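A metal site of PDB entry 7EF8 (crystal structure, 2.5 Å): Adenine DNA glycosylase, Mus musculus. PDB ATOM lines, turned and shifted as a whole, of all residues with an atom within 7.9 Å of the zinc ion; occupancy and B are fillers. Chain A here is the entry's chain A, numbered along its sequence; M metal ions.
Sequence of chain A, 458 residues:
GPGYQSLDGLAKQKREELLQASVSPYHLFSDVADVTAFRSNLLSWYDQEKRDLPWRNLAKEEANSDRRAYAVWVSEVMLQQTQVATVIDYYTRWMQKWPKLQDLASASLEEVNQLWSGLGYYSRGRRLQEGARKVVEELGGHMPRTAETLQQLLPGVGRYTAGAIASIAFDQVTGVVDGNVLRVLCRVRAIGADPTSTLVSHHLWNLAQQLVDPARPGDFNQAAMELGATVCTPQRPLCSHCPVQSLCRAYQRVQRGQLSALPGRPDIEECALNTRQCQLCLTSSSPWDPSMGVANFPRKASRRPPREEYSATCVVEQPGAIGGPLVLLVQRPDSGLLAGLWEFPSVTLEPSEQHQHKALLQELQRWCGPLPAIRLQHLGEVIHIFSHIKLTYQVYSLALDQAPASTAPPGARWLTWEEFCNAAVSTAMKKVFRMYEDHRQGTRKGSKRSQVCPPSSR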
ATOM      1  N   VAL A  23       7.395 -11.892 -20.976  1.00  0.00           N
ATOM      2  CA  VAL A  23       6.061 -12.402 -20.678  1.00  0.00           C
ATOM      3  C   VAL A  23       5.065 -11.640 -21.557  1.00  0.00           C
ATOM      4  O   VAL A  23       5.392 -10.628 -22.185  1.00  0.00           O
ATOM      5  CB  VAL A  23       5.700 -12.267 -19.178  1.00  0.00           C
ATOM      6  CG1 VAL A  23       4.406 -12.974 -18.842  1.00  0.00           C
ATOM      7  CG2 VAL A  23       6.805 -12.818 -18.286  1.00  0.00           C
ATOM      8  N   SER A  24       3.837 -12.166 -21.644  1.00  0.00           N
ATOM      9  CA  SER A  24       2.751 -11.551 -22.411  1.00  0.00           C
ATOM     10  C   SER A  24       2.179 -10.346 -21.676  1.00  0.00           C
ATOM     11  O   SER A  24       2.338 -10.210 -20.457  1.00  0.00           O
ATOM     12  CB  SER A  24       1.653 -12.580 -22.655  1.00  0.00           C
ATOM     13  OG  SER A  24       0.397 -12.094 -22.226  1.00  0.00           O
ATOM     14  N   TYR A  26      -1.053  -9.894 -21.434  1.00  0.00           N
ATOM     15  CA  TYR A  26      -2.226 -10.421 -20.744  1.00  0.00           C
ATOM     16  C   TYR A  26      -1.898 -10.792 -19.303  1.00  0.00           C
ATOM     17  O   TYR A  26      -2.809 -10.957 -18.486  1.00  0.00           O
ATOM     18  CB  TYR A  26      -2.756 -11.631 -21.530  1.00  0.00           C
ATOM     19  CG  TYR A  26      -3.826 -12.467 -20.860  1.00  0.00           C
ATOM     20  CD1 TYR A  26      -3.494 -13.571 -20.088  1.00  0.00           C
ATOM     21  CD2 TYR A  26      -5.173 -12.175 -21.030  1.00  0.00           C
ATOM     22  CE1 TYR A  26      -4.458 -14.353 -19.502  1.00  0.00           C
ATOM     23  CE2 TYR A  26      -6.162 -12.957 -20.440  1.00  0.00           C
ATOM     24  CZ  TYR A  26      -5.789 -14.044 -19.667  1.00  0.00           C
ATOM     25  OH  TYR A  26      -6.754 -14.826 -19.081  1.00  0.00           O
ATOM     26  N   HIS A  27      -0.603 -10.874 -19.023  1.00  0.00           N
ATOM     27  CA  HIS A  27      -0.045 -11.231 -17.737  1.00  0.00           C
ATOM     28  C   HIS A  27       0.624 -10.082 -16.998  1.00  0.00           C
ATOM     29  O   HIS A  27       1.113 -10.257 -15.905  1.00  0.00           O
ATOM     30  CB  HIS A  27       1.002 -12.307 -17.915  1.00  0.00           C
ATOM     31  CG  HIS A  27       0.454 -13.684 -18.012  1.00  0.00           C
ATOM     32  ND1 HIS A  27      -0.772 -14.034 -17.516  1.00  0.00           N
ATOM     33  CD2 HIS A  27       0.972 -14.807 -18.556  1.00  0.00           C
ATOM     34  CE1 HIS A  27      -0.988 -15.318 -17.744  1.00  0.00           C
ATOM     35  NE2 HIS A  27       0.051 -15.800 -18.382  1.00  0.00           N
ATOM     36  N   ARG A 189      -4.397 -10.951 -13.168  1.00  0.00           N
ATOM     37  CA  ARG A 189      -3.604 -11.245 -14.359  1.00  0.00           C
ATOM     38  C   ARG A 189      -3.692 -12.707 -14.765  1.00  0.00           C
ATOM     39  O   ARG A 189      -2.903 -13.153 -15.606  1.00  0.00           O
ATOM     40  CB  ARG A 189      -2.147 -10.827 -14.133  1.00  0.00           C
ATOM     41  CG  ARG A 189      -1.937  -9.306 -14.104  1.00  0.00           C
ATOM     42  CD  ARG A 189      -2.131  -8.682 -15.478  1.00  0.00           C
ATOM     43  NE  ARG A 189      -3.535  -8.455 -15.823  1.00  0.00           N
ATOM     44  CZ  ARG A 189      -4.008  -7.307 -16.291  1.00  0.00           C
ATOM     45  NH1 ARG A 189      -3.203  -6.280 -16.488  1.00  0.00           N
ATOM     46  NH2 ARG A 189      -5.300  -7.196 -16.578  1.00  0.00           N
ATOM     47  N   ALA A 190      -4.625 -13.461 -14.182  1.00  0.00           N
ATOM     48  CA  ALA A 190      -4.959 -14.814 -14.629  1.00  0.00           C
ATOM     49  C   ALA A 190      -3.744 -15.746 -14.618  1.00  0.00           C
ATOM     50  O   ALA A 190      -3.507 -16.501 -15.561  1.00  0.00           O
ATOM     51  CB  ALA A 190      -5.610 -14.794 -16.019  1.00  0.00           C
ATOM     52  N   ILE A 191      -2.973 -15.693 -13.541  1.00  0.00           N
ATOM     53  CA  ILE A 191      -1.822 -16.583 -13.389  1.00  0.00           C
ATOM     54  C   ILE A 191      -2.323 -17.924 -12.856  1.00  0.00           C
ATOM     55  O   ILE A 191      -2.866 -18.008 -11.752  1.00  0.00           O
ATOM     56  CB  ILE A 191      -0.771 -15.972 -12.445  1.00  0.00           C
ATOM     57  CG1 ILE A 191      -0.128 -14.741 -13.089  1.00  0.00           C
ATOM     58  CG2 ILE A 191       0.277 -17.016 -12.111  1.00  0.00           C
ATOM     59  CD1 ILE A 191       0.853 -14.034 -12.199  1.00  0.00           C
ATOM     60  N   GLY A 192      -2.140 -18.970 -13.659  1.00  0.00           N
ATOM     61  CA  GLY A 192      -2.630 -20.286 -13.300  1.00  0.00           C
ATOM     62  C   GLY A 192      -1.540 -21.290 -12.985  1.00  0.00           C
ATOM     63  O   GLY A 192      -1.829 -22.468 -12.744  1.00  0.00           O
ATOM     64  N   CYS A 271      -4.614 -14.888 -24.024  1.00  0.00           N
ATOM     65  CA  CYS A 271      -3.173 -15.045 -23.873  1.00  0.00           C
ATOM     66  C   CYS A 271      -2.572 -15.777 -25.060  1.00  0.00           C
ATOM     67  O   CYS A 271      -3.269 -16.460 -25.830  1.00  0.00           O
ATOM     68  CB  CYS A 271      -2.849 -15.798 -22.581  1.00  0.00           C
ATOM     69  SG  CYS A 271      -1.094 -15.870 -22.194  1.00  0.00           S
ATOM     70  N   ALA A 272      -1.263 -15.648 -25.209  1.00  0.00           N
ATOM     71  CA  ALA A 272      -0.535 -16.296 -26.290  1.00  0.00           C
ATOM     72  C   ALA A 272       0.077 -17.609 -25.832  1.00  0.00           C
ATOM     73  O   ALA A 272      -0.290 -18.678 -26.314  1.00  0.00           O
ATOM     74  CB  ALA A 272       0.551 -15.366 -26.826  1.00  0.00           C
ATOM     75  N   CYS A 278       3.729 -21.575 -22.647  1.00  0.00           N
ATOM     76  CA  CYS A 278       3.914 -20.463 -21.710  1.00  0.00           C
ATOM     77  C   CYS A 278       4.436 -20.952 -20.368  1.00  0.00           C
ATOM     78  O   CYS A 278       4.817 -22.113 -20.223  1.00  0.00           O
ATOM     79  CB  CYS A 278       2.603 -19.702 -21.524  1.00  0.00           C
ATOM     80  SG  CYS A 278       2.762 -18.140 -20.611  1.00  0.00           S
ATOM     81  N   GLN A 279       4.432 -20.060 -19.378  1.00  0.00           N
ATOM     82  CA  GLN A 279       4.931 -20.395 -18.046  1.00  0.00           C
ATOM     83  C   GLN A 279       4.092 -19.820 -16.918  1.00  0.00           C
ATOM     84  O   GLN A 279       4.371 -20.121 -15.761  1.00  0.00           O
ATOM     85  CB  GLN A 279       6.390 -19.923 -17.896  1.00  0.00           C
ATOM     86  CG  GLN A 279       6.558 -18.420 -18.027  1.00  0.00           C
ATOM     87  CD  GLN A 279       8.001 -18.010 -18.251  1.00  0.00           C
ATOM     88  OE1 GLN A 279       8.318 -16.824 -18.349  1.00  0.00           O
ATOM     89  NE2 GLN A 279       8.887 -18.999 -18.336  1.00  0.00           N
ATOM     90  N   LEU A 280       3.075 -19.000 -17.216  1.00  0.00           N
ATOM     91  CA  LEU A 280       2.223 -18.425 -16.190  1.00  0.00           C
ATOM     92  C   LEU A 280       0.766 -18.870 -16.274  1.00  0.00           C
ATOM     93  O   LEU A 280       0.030 -18.665 -15.303  1.00  0.00           O
ATOM     94  CB  LEU A 280       2.274 -16.891 -16.247  1.00  0.00           C
ATOM     95  CG  LEU A 280       3.636 -16.239 -16.012  1.00  0.00           C
ATOM     96  CD1 LEU A 280       3.488 -14.733 -15.952  1.00  0.00           C
ATOM     97  CD2 LEU A 280       4.270 -16.772 -14.745  1.00  0.00           C
ATOM     98  N   CYS A 281       0.337 -19.448 -17.387  1.00  0.00           N
ATOM     99  CA  CYS A 281      -1.026 -19.941 -17.509  1.00  0.00           C
ATOM    100  C   CYS A 281      -1.138 -21.312 -16.830  1.00  0.00           C
ATOM    101  O   CYS A 281      -0.213 -21.773 -16.164  1.00  0.00           O
ATOM    102  CB  CYS A 281      -1.440 -19.994 -18.979  1.00  0.00           C
ATOM    103  SG  CYS A 281      -1.726 -18.395 -19.752  1.00  0.00           S
ATOM    104  N   LEU A 282      -2.279 -21.970 -17.007  1.00  0.00           N
ATOM    105  CA  LEU A 282      -2.481 -23.295 -16.440  1.00  0.00           C
ATOM    106  C   LEU A 282      -1.779 -24.334 -17.312  1.00  0.00           C
ATOM    107  O   LEU A 282      -1.950 -24.364 -18.535  1.00  0.00           O
ATOM    108  CB  LEU A 282      -3.970 -23.607 -16.323  1.00  0.00           C
ATOM    109  CG  LEU A 282      -4.701 -22.886 -15.198  1.00  0.00           C
ATOM    110  CD1 LEU A 282      -5.924 -22.152 -15.732  1.00  0.00           C
ATOM    111  CD2 LEU A 282      -5.104 -23.864 -14.104  1.00  0.00           C
HETATM  112 ZN    ZN M   1       0.432 -17.540 -20.249  1.00  0.00          ZN
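SG of Cys 271 sits close to SG of Cys 281, 3.6 Å away. SG of Cys 278 sits close to N of Leu 280, at 3.5 Å. A ring nitrogen (ND1) of His 27 sits at hydrogen-bond distance from the backbone carbonyl oxygen (O) of Arg 189 (3.0 Å).
Within 4 Å of the zinc ion: His 27, Cys 271, Cys 278 and Cys 281.
The zinc ion is bound by SG of Cys 281 (2.4 Å), SG of Cys 278 (2.4 Å) and NE2 of His 27 (2.6 Å). The zinc ion has three donor atoms within binding distance. Slightly farther from the zinc ion lies the side-chain sulfur (SG) of Cys 271 (3.0 Å).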
